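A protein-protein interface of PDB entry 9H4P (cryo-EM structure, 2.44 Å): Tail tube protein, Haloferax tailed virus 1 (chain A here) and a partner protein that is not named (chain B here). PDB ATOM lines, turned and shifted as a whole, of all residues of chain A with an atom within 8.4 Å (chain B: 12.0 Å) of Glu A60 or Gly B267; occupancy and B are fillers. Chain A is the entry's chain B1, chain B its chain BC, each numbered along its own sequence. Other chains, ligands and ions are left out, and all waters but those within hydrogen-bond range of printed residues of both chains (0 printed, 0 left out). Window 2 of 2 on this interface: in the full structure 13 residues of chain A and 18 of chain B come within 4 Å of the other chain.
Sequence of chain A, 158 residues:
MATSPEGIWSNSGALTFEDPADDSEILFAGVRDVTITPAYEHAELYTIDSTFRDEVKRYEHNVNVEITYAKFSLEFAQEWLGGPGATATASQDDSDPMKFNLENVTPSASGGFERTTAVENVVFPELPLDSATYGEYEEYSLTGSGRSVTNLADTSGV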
ATOM      1  N   PRO A  38     -13.957  15.600  16.222  1.00  0.00           N
ATOM      2  CA  PRO A  38     -14.609  15.773  14.920  1.00  0.00           C
ATOM      3  C   PRO A  38     -16.119  15.938  15.103  1.00  0.00           C
ATOM      4  O   PRO A  38     -16.747  15.242  15.909  1.00  0.00           O
ATOM      5  CB  PRO A  38     -14.268  14.493  14.131  1.00  0.00           C
ATOM      6  CG  PRO A  38     -13.903  13.480  15.205  1.00  0.00           C
ATOM      7  CD  PRO A  38     -13.261  14.302  16.312  1.00  0.00           C
ATOM      8  N   ALA A  39     -16.665  16.890  14.338  1.00  0.00           N
ATOM      9  CA  ALA A  39     -18.055  17.297  14.439  1.00  0.00           C
ATOM     10  C   ALA A  39     -18.596  17.625  13.051  1.00  0.00           C
ATOM     11  O   ALA A  39     -17.863  18.089  12.174  1.00  0.00           O
ATOM     12  CB  ALA A  39     -18.174  18.491  15.364  1.00  0.00           C
ATOM     13  N   TYR A  40     -19.900  17.385  12.889  1.00  0.00           N
ATOM     14  CA  TYR A  40     -20.675  17.924  11.785  1.00  0.00           C
ATOM     15  C   TYR A  40     -21.937  18.546  12.380  1.00  0.00           C
ATOM     16  O   TYR A  40     -22.402  18.119  13.443  1.00  0.00           O
ATOM     17  CB  TYR A  40     -21.098  16.804  10.826  1.00  0.00           C
ATOM     18  CG  TYR A  40     -20.027  15.984  10.143  1.00  0.00           C
ATOM     19  CD1 TYR A  40     -19.400  14.918  10.788  1.00  0.00           C
ATOM     20  CD2 TYR A  40     -19.725  16.205   8.801  1.00  0.00           C
ATOM     21  CE1 TYR A  40     -18.472  14.124  10.129  1.00  0.00           C
ATOM     22  CE2 TYR A  40     -18.801  15.418   8.126  1.00  0.00           C
ATOM     23  CZ  TYR A  40     -18.173  14.377   8.796  1.00  0.00           C
ATOM     24  OH  TYR A  40     -17.244  13.607   8.156  1.00  0.00           O
ATOM     25  N   GLU A  41     -22.490  19.544  11.683  1.00  0.00           N
ATOM     26  CA  GLU A  41     -23.863  19.944  11.950  1.00  0.00           C
ATOM     27  C   GLU A  41     -24.794  18.889  11.344  1.00  0.00           C
ATOM     28  O   GLU A  41     -24.494  18.339  10.281  1.00  0.00           O
ATOM     29  CB  GLU A  41     -24.141  21.337  11.378  1.00  0.00           C
ATOM     30  CG  GLU A  41     -23.345  22.458  12.032  1.00  0.00           C
ATOM     31  CD  GLU A  41     -23.624  22.701  13.505  1.00  0.00           C
ATOM     32  OE1 GLU A  41     -24.695  22.291  13.992  1.00  0.00           O
ATOM     33  OE2 GLU A  41     -22.765  23.303  14.166  1.00  0.00           O
ATOM     34  N   HIS A  42     -25.910  18.603  12.035  1.00  0.00           N
ATOM     35  CA  HIS A  42     -26.927  17.683  11.538  1.00  0.00           C
ATOM     36  C   HIS A  42     -28.194  18.455  11.177  1.00  0.00           C
ATOM     37  O   HIS A  42     -28.748  19.166  12.018  1.00  0.00           O
ATOM     38  CB  HIS A  42     -27.242  16.582  12.573  1.00  0.00           C
ATOM     39  CG  HIS A  42     -26.243  15.471  12.614  1.00  0.00           C
ATOM     40  ND1 HIS A  42     -26.452  14.298  13.330  1.00  0.00           N
ATOM     41  CD2 HIS A  42     -25.035  15.337  12.016  1.00  0.00           C
ATOM     42  CE1 HIS A  42     -25.408  13.501  13.178  1.00  0.00           C
ATOM     43  NE2 HIS A  42     -24.523  14.118  12.374  1.00  0.00           N
ATOM     44  N   LYS A  57     -28.867  14.525   7.915  1.00  0.00           N
ATOM     45  CA  LYS A  57     -27.747  14.807   7.020  1.00  0.00           C
ATOM     46  C   LYS A  57     -26.637  15.588   7.731  1.00  0.00           C
ATOM     47  O   LYS A  57     -26.916  16.541   8.463  1.00  0.00           O
ATOM     48  CB  LYS A  57     -28.233  15.585   5.788  1.00  0.00           C
ATOM     49  CG  LYS A  57     -28.967  14.766   4.731  1.00  0.00           C
ATOM     50  CD  LYS A  57     -28.105  13.685   4.099  1.00  0.00           C
ATOM     51  CE  LYS A  57     -28.695  13.133   2.821  1.00  0.00           C
ATOM     52  NZ  LYS A  57     -27.701  12.362   2.039  1.00  0.00           N
ATOM     53  N   ARG A  58     -25.379  15.193   7.465  1.00  0.00           N
ATOM     54  CA  ARG A  58     -24.173  15.874   7.930  1.00  0.00           C
ATOM     55  C   ARG A  58     -23.843  17.055   7.016  1.00  0.00           C
ATOM     56  O   ARG A  58     -23.928  16.932   5.791  1.00  0.00           O
ATOM     57  CB  ARG A  58     -22.956  14.940   7.872  1.00  0.00           C
ATOM     58  CG  ARG A  58     -23.087  13.665   8.694  1.00  0.00           C
ATOM     59  CD  ARG A  58     -21.759  12.978   8.973  1.00  0.00           C
ATOM     60  NE  ARG A  58     -21.138  12.292   7.838  1.00  0.00           N
ATOM     61  CZ  ARG A  58     -20.258  11.294   7.936  1.00  0.00           C
ATOM     62  NH1 ARG A  58     -19.758  10.742   6.843  1.00  0.00           N
ATOM     63  NH2 ARG A  58     -19.880  10.842   9.121  1.00  0.00           N
ATOM     64  N   TYR A  59     -23.429  18.179   7.626  1.00  0.00           N
ATOM     65  CA  TYR A  59     -22.901  19.331   6.902  1.00  0.00           C
ATOM     66  C   TYR A  59     -21.865  20.068   7.757  1.00  0.00           C
ATOM     67  O   TYR A  59     -21.769  19.811   8.961  1.00  0.00           O
ATOM     68  CB  TYR A  59     -24.038  20.231   6.392  1.00  0.00           C
ATOM     69  CG  TYR A  59     -24.851  20.996   7.415  1.00  0.00           C
ATOM     70  CD1 TYR A  59     -25.923  20.402   8.078  1.00  0.00           C
ATOM     71  CD2 TYR A  59     -24.596  22.341   7.668  1.00  0.00           C
ATOM     72  CE1 TYR A  59     -26.694  21.112   8.991  1.00  0.00           C
ATOM     73  CE2 TYR A  59     -25.357  23.064   8.579  1.00  0.00           C
ATOM     74  CZ  TYR A  59     -26.410  22.447   9.240  1.00  0.00           C
ATOM     75  OH  TYR A  59     -27.157  23.148  10.144  1.00  0.00           O
ATOM     76  N   GLU A  60     -21.086  20.966   7.116  1.00  0.00           N
ATOM     77  CA  GLU A  60     -20.201  21.927   7.774  1.00  0.00           C
ATOM     78  C   GLU A  60     -19.263  21.228   8.768  1.00  0.00           C
ATOM     79  O   GLU A  60     -19.328  21.473   9.977  1.00  0.00           O
ATOM     80  CB  GLU A  60     -21.042  23.048   8.408  1.00  0.00           C
ATOM     81  CG  GLU A  60     -20.265  24.296   8.807  1.00  0.00           C
ATOM     82  CD  GLU A  60     -21.097  25.337   9.534  1.00  0.00           C
ATOM     83  OE1 GLU A  60     -22.263  25.544   9.145  1.00  0.00           O
ATOM     84  OE2 GLU A  60     -20.578  25.937  10.486  1.00  0.00           O
ATOM     85  N   HIS A  61     -18.393  20.353   8.239  1.00  0.00           N
ATOM     86  CA  HIS A  61     -17.487  19.544   9.046  1.00  0.00           C
ATOM     87  C   HIS A  61     -16.439  20.421   9.737  1.00  0.00           C
ATOM     88  O   HIS A  61     -15.992  21.428   9.182  1.00  0.00           O
ATOM     89  CB  HIS A  61     -16.831  18.440   8.198  1.00  0.00           C
ATOM     90  CG  HIS A  61     -16.002  17.488   8.998  1.00  0.00           C
ATOM     91  ND1 HIS A  61     -16.540  16.669   9.982  1.00  0.00           N
ATOM     92  CD2 HIS A  61     -14.674  17.230   8.976  1.00  0.00           C
ATOM     93  CE1 HIS A  61     -15.582  15.936  10.517  1.00  0.00           C
ATOM     94  NE2 HIS A  61     -14.425  16.267   9.919  1.00  0.00           N
ATOM     95  N   ASN A  62     -16.038  19.980  10.939  1.00  0.00           N
ATOM     96  CA  ASN A  62     -15.155  20.706  11.836  1.00  0.00           C
ATOM     97  C   ASN A  62     -14.435  19.676  12.709  1.00  0.00           C
ATOM     98  O   ASN A  62     -14.964  18.585  12.932  1.00  0.00           O
ATOM     99  CB  ASN A  62     -15.987  21.685  12.676  1.00  0.00           C
ATOM    100  CG  ASN A  62     -15.203  22.507  13.680  1.00  0.00           C
ATOM    101  OD1 ASN A  62     -13.994  22.698  13.552  1.00  0.00           O
ATOM    102  ND2 ASN A  62     -15.890  23.012  14.694  1.00  0.00           N
ATOM    103  N   VAL A  63     -13.229  20.014  13.194  1.00  0.00           N
ATOM    104  CA  VAL A  63     -12.592  19.248  14.261  1.00  0.00           C
ATOM    105  C   VAL A  63     -12.224  20.229  15.375  1.00  0.00           C
ATOM    106  O   VAL A  63     -11.228  20.948  15.258  1.00  0.00           O
ATOM    107  CB  VAL A  63     -11.361  18.431  13.790  1.00  0.00           C
ATOM    108  CG1 VAL A  63     -10.734  17.610  14.919  1.00  0.00           C
ATOM    109  CG2 VAL A  63     -11.661  17.534  12.589  1.00  0.00           C
ATOM    110  N   ASN A  64     -13.041  20.262  16.437  1.00  0.00           N
ATOM    111  CA  ASN A  64     -12.729  21.076  17.604  1.00  0.00           C
ATOM    112  C   ASN A  64     -11.489  20.508  18.294  1.00  0.00           C
ATOM    113  O   ASN A  64     -11.476  19.344  18.698  1.00  0.00           O
ATOM    114  CB  ASN A  64     -13.904  21.146  18.586  1.00  0.00           C
ATOM    115  CG  ASN A  64     -15.128  21.832  18.012  1.00  0.00           C
ATOM    116  OD1 ASN A  64     -16.047  21.171  17.530  1.00  0.00           O
ATOM    117  ND2 ASN A  64     -15.154  23.155  18.054  1.00  0.00           N
ATOM    118  N   GLY A 146      -9.595  22.232  13.391  1.00  0.00           N
ATOM    119  CA  GLY A 146      -8.973  21.518  12.282  1.00  0.00           C
ATOM    120  C   GLY A 146      -9.953  21.300  11.127  1.00  0.00           C
ATOM    121  O   GLY A 146     -11.168  21.420  11.305  1.00  0.00           O
ATOM    122  N   ARG A 147      -9.407  20.974   9.947  1.00  0.00           N
ATOM    123  CA  ARG A 147     -10.206  20.735   8.752  1.00  0.00           C
ATOM    124  C   ARG A 147     -10.813  19.327   8.766  1.00  0.00           C
ATOM    125  O   ARG A 147     -12.009  19.171   8.496  1.00  0.00           O
ATOM    126  CB  ARG A 147      -9.377  21.009   7.492  1.00  0.00           C
ATOM    127  CG  ARG A 147     -10.130  20.748   6.196  1.00  0.00           C
ATOM    128  CD  ARG A 147      -9.268  21.105   5.002  1.00  0.00           C
ATOM    129  NE  ARG A 147      -9.946  20.877   3.730  1.00  0.00           N
ATOM    130  CZ  ARG A 147      -9.886  19.765   2.995  1.00  0.00           C
ATOM    131  NH1 ARG A 147     -10.548  19.706   1.851  1.00  0.00           N
ATOM    132  NH2 ARG A 147      -9.176  18.720   3.389  1.00  0.00           N
ATOM    133  N   GLU B 211     -36.004  19.580   0.196  1.00  0.00           N
ATOM    134  CA  GLU B 211     -34.564  19.466  -0.001  1.00  0.00           C
ATOM    135  C   GLU B 211     -34.261  18.159  -0.741  1.00  0.00           C
ATOM    136  O   GLU B 211     -34.609  17.083  -0.252  1.00  0.00           O
ATOM    137  CB  GLU B 211     -33.840  19.621   1.345  1.00  0.00           C
ATOM    138  CG  GLU B 211     -34.202  20.919   2.062  1.00  0.00           C
ATOM    139  CD  GLU B 211     -33.462  21.259   3.344  1.00  0.00           C
ATOM    140  OE1 GLU B 211     -32.259  20.974   3.434  1.00  0.00           O
ATOM    141  OE2 GLU B 211     -34.098  21.806   4.258  1.00  0.00           O
ATOM    142  N   THR B 212     -33.649  18.256  -1.938  1.00  0.00           N
ATOM    143  CA  THR B 212     -33.250  17.081  -2.712  1.00  0.00           C
ATOM    144  C   THR B 212     -31.927  16.544  -2.161  1.00  0.00           C
ATOM    145  O   THR B 212     -30.917  17.251  -2.189  1.00  0.00           O
ATOM    146  CB  THR B 212     -33.068  17.372  -4.214  1.00  0.00           C
ATOM    147  OG1 THR B 212     -32.122  18.431  -4.395  1.00  0.00           O
ATOM    148  CG2 THR B 212     -34.347  17.709  -4.953  1.00  0.00           C
ATOM    149  N   LEU B 213     -31.929  15.285  -1.689  1.00  0.00           N
ATOM    150  CA  LEU B 213     -30.804  14.725  -0.945  1.00  0.00           C
ATOM    151  C   LEU B 213     -30.011  13.682  -1.741  1.00  0.00           C
ATOM    152  O   LEU B 213     -28.833  13.468  -1.449  1.00  0.00           O
ATOM    153  CB  LEU B 213     -31.307  14.121   0.374  1.00  0.00           C
ATOM    154  CG  LEU B 213     -32.005  15.063   1.362  1.00  0.00           C
ATOM    155  CD1 LEU B 213     -32.328  14.327   2.654  1.00  0.00           C
ATOM    156  CD2 LEU B 213     -31.161  16.292   1.677  1.00  0.00           C
ATOM    157  N   ILE B 216     -29.404  13.892  -7.240  1.00  0.00           N
ATOM    158  CA  ILE B 216     -29.692  15.322  -7.264  1.00  0.00           C
ATOM    159  C   ILE B 216     -29.719  15.877  -8.694  1.00  0.00           C
ATOM    160  O   ILE B 216     -30.708  16.525  -9.048  1.00  0.00           O
ATOM    161  CB  ILE B 216     -28.775  16.106  -6.295  1.00  0.00           C
ATOM    162  CG1 ILE B 216     -29.151  15.828  -4.834  1.00  0.00           C
ATOM    163  CG2 ILE B 216     -28.768  17.600  -6.609  1.00  0.00           C
ATOM    164  CD1 ILE B 216     -28.136  16.305  -3.813  1.00  0.00           C
ATOM    165  N   VAL B 263     -31.117  26.362  -4.356  1.00  0.00           N
ATOM    166  CA  VAL B 263     -30.263  27.090  -3.426  1.00  0.00           C
ATOM    167  C   VAL B 263     -29.177  26.151  -2.894  1.00  0.00           C
ATOM    168  O   VAL B 263     -29.470  25.102  -2.316  1.00  0.00           O
ATOM    169  CB  VAL B 263     -31.073  27.779  -2.299  1.00  0.00           C
ATOM    170  CG1 VAL B 263     -30.207  28.252  -1.135  1.00  0.00           C
ATOM    171  CG2 VAL B 263     -31.899  28.948  -2.832  1.00  0.00           C
ATOM    172  N   HIS B 264     -27.923  26.580  -3.093  1.00  0.00           N
ATOM    173  CA  HIS B 264     -26.727  25.901  -2.622  1.00  0.00           C
ATOM    174  C   HIS B 264     -26.119  26.714  -1.478  1.00  0.00           C
ATOM    175  O   HIS B 264     -25.892  27.917  -1.631  1.00  0.00           O
ATOM    176  CB  HIS B 264     -25.733  25.777  -3.790  1.00  0.00           C
ATOM    177  CG  HIS B 264     -26.171  24.872  -4.895  1.00  0.00           C
ATOM    178  ND1 HIS B 264     -27.132  25.225  -5.840  1.00  0.00           N
ATOM    179  CD2 HIS B 264     -25.768  23.624  -5.216  1.00  0.00           C
ATOM    180  CE1 HIS B 264     -27.302  24.222  -6.684  1.00  0.00           C
ATOM    181  NE2 HIS B 264     -26.472  23.231  -6.323  1.00  0.00           N
ATOM    182  N   GLN B 265     -25.865  26.054  -0.339  1.00  0.00           N
ATOM    183  CA  GLN B 265     -25.317  26.721   0.835  1.00  0.00           C
ATOM    184  C   GLN B 265     -23.915  26.190   1.128  1.00  0.00           C
ATOM    185  O   GLN B 265     -23.651  25.004   0.922  1.00  0.00           O
ATOM    186  CB  GLN B 265     -26.239  26.555   2.046  1.00  0.00           C
ATOM    187  CG  GLN B 265     -27.508  27.392   1.944  1.00  0.00           C
ATOM    188  CD  GLN B 265     -28.504  27.079   3.035  1.00  0.00           C
ATOM    189  OE1 GLN B 265     -29.533  26.448   2.797  1.00  0.00           O
ATOM    190  NE2 GLN B 265     -28.209  27.531   4.245  1.00  0.00           N
ATOM    191  N   ALA B 266     -23.037  27.087   1.605  1.00  0.00           N
ATOM    192  CA  ALA B 266     -21.663  26.754   1.963  1.00  0.00           C
ATOM    193  C   ALA B 266     -21.641  25.582   2.949  1.00  0.00           C
ATOM    194  O   ALA B 266     -22.330  25.620   3.971  1.00  0.00           O
ATOM    195  CB  ALA B 266     -20.963  27.971   2.531  1.00  0.00           C
ATOM    196  N   GLY B 267     -20.870  24.535   2.613  1.00  0.00           N
ATOM    197  CA  GLY B 267     -20.648  23.402   3.503  1.00  0.00           C
ATOM    198  C   GLY B 267     -21.751  22.335   3.503  1.00  0.00           C
ATOM    199  O   GLY B 267     -21.653  21.383   4.278  1.00  0.00           O
ATOM    200  N   ARG B 268     -22.783  22.468   2.646  1.00  0.00           N
ATOM    201  CA  ARG B 268     -23.867  21.486   2.569  1.00  0.00           C
ATOM    202  C   ARG B 268     -23.775  20.685   1.267  1.00  0.00           C
ATOM    203  O   ARG B 268     -23.691  21.270   0.183  1.00  0.00           O
ATOM    204  CB  ARG B 268     -25.245  22.151   2.692  1.00  0.00           C
ATOM    205  CG  ARG B 268     -25.421  22.983   3.955  1.00  0.00           C
ATOM    206  CD  ARG B 268     -26.870  23.306   4.268  1.00  0.00           C
ATOM    207  NE  ARG B 268     -26.944  24.162   5.445  1.00  0.00           N
ATOM    208  CZ  ARG B 268     -28.045  24.445   6.139  1.00  0.00           C
ATOM    209  NH1 ARG B 268     -27.965  25.242   7.190  1.00  0.00           N
ATOM    210  NH2 ARG B 268     -29.216  23.938   5.796  1.00  0.00           N
ATOM    211  N   GLY B 269     -23.838  19.347   1.388  1.00  0.00           N
ATOM    212  CA  GLY B 269     -23.675  18.438   0.259  1.00  0.00           C
ATOM    213  C   GLY B 269     -24.953  18.170  -0.544  1.00  0.00           C
ATOM    214  O   GLY B 269     -25.030  17.140  -1.214  1.00  0.00           O
ATOM    215  N   TRP B 270     -25.936  19.089  -0.494  1.00  0.00           N
ATOM    216  CA  TRP B 270     -27.234  18.900  -1.138  1.00  0.00           C
ATOM    217  C   TRP B 270     -27.857  20.243  -1.532  1.00  0.00           C
ATOM    218  O   TRP B 270     -27.305  21.300  -1.220  1.00  0.00           O
ATOM    219  CB  TRP B 270     -28.155  18.069  -0.229  1.00  0.00           C
ATOM    220  CG  TRP B 270     -28.678  18.802   0.972  1.00  0.00           C
ATOM    221  CD1 TRP B 270     -29.805  19.571   1.026  1.00  0.00           C
ATOM    222  CD2 TRP B 270     -28.113  18.823   2.303  1.00  0.00           C
ATOM    223  NE1 TRP B 270     -29.977  20.070   2.288  1.00  0.00           N
ATOM    224  CE2 TRP B 270     -28.963  19.626   3.100  1.00  0.00           C
ATOM    225  CE3 TRP B 270     -26.989  18.241   2.910  1.00  0.00           C
ATOM    226  CZ2 TRP B 270     -28.717  19.858   4.461  1.00  0.00           C
ATOM    227  CZ3 TRP B 270     -26.745  18.475   4.251  1.00  0.00           C
ATOM    228  CH2 TRP B 270     -27.600  19.272   5.019  1.00  0.00           C
ATOM    229  N   VAL B 271     -29.020  20.190  -2.205  1.00  0.00           N
ATOM    230  CA  VAL B 271     -29.688  21.375  -2.735  1.00  0.00           C
ATOM    231  C   VAL B 271     -31.001  21.591  -1.976  1.00  0.00           C
ATOM    232  O   VAL B 271     -31.762  20.644  -1.757  1.00  0.00           O
ATOM    233  CB  VAL B 271     -29.901  21.279  -4.267  1.00  0.00           C
ATOM    234  CG1 VAL B 271     -30.485  22.558  -4.866  1.00  0.00           C
ATOM    235  CG2 VAL B 271     -28.628  20.888  -5.013  1.00  0.00           C
ATOM    236  N   THR B 272     -31.235  22.848  -1.563  1.00  0.00           N
ATOM    237  CA  THR B 272     -32.516  23.295  -1.028  1.00  0.00           C
ATOM    238  C   THR B 272     -33.362  23.888  -2.159  1.00  0.00           C
ATOM    239  O   THR B 272     -32.848  24.635  -2.995  1.00  0.00           O
ATOM    240  CB  THR B 272     -32.315  24.350   0.073  1.00  0.00           C
ATOM    241  OG1 THR B 272     -31.510  23.784   1.107  1.00  0.00           O
ATOM    242  CG2 THR B 272     -33.601  24.881   0.673  1.00  0.00           C
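The backbone carbonyl oxygen (O) of Gly B267 lies within hydrogen-bond range of the backbone NH (N) of Glu A60 (2.9 Å).
OE1 of Glu B211 is in hydrogen-bond range of NE1 of Trp B270 (2.7 Å).
The backbone carbonyl oxygen (O) of Tyr A59 sits at hydrogen-bond distance from the backbone NH (N) of Glu A41, 2.8 Å away.
Among the printed residues, pairs that only touch across the chains: Tyr A59 with Gly B267 (3.4 Å), Arg A58 with Trp B270 (3.6 Å), Lys A57 with Trp B270 (3.6 Å), Tyr A59 with Trp B270 (3.7 Å), Tyr A59 with Arg B268 (3.7 Å) and Lys A57 with Leu B213 (3.7 Å).
No residue of chain B comes within 4 Å of Tyr A40.
Of the printed residues of chain B, Lys A57 touches Leu B213 and Trp B270.
Printed residues of chain B within 4 Å of Arg A58: Trp B270 (3.6 Å).
Tyr A59 touches three residues of chain B.
Glu A60 touches one residue of chain B.
No residue of chain B comes within 4 Å of His A61.
No residue of chain B comes within 4 Å of Asn A62.
The nearest printed residue of chain A that does not touch Gly B267 is Arg A58 (5.2 Å).
Of the 15 printed residues of chain A, 4 touch a printed residue of chain B.
Printed residues of chain A that touch a printed residue of chain B: Lys A57, Arg A58, Tyr A59 and Glu A60.
Hydrophobic or aromatic side chains of chain A that line the printed part of chain B: Tyr A59.
Of the 14 printed residues of chain B, 4 touch a printed residue of chain A.
Among the printed residues, no Asp or Glu carboxylate lies within 4 Å of a Lys or Arg side-chain nitrogen of the other chain.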
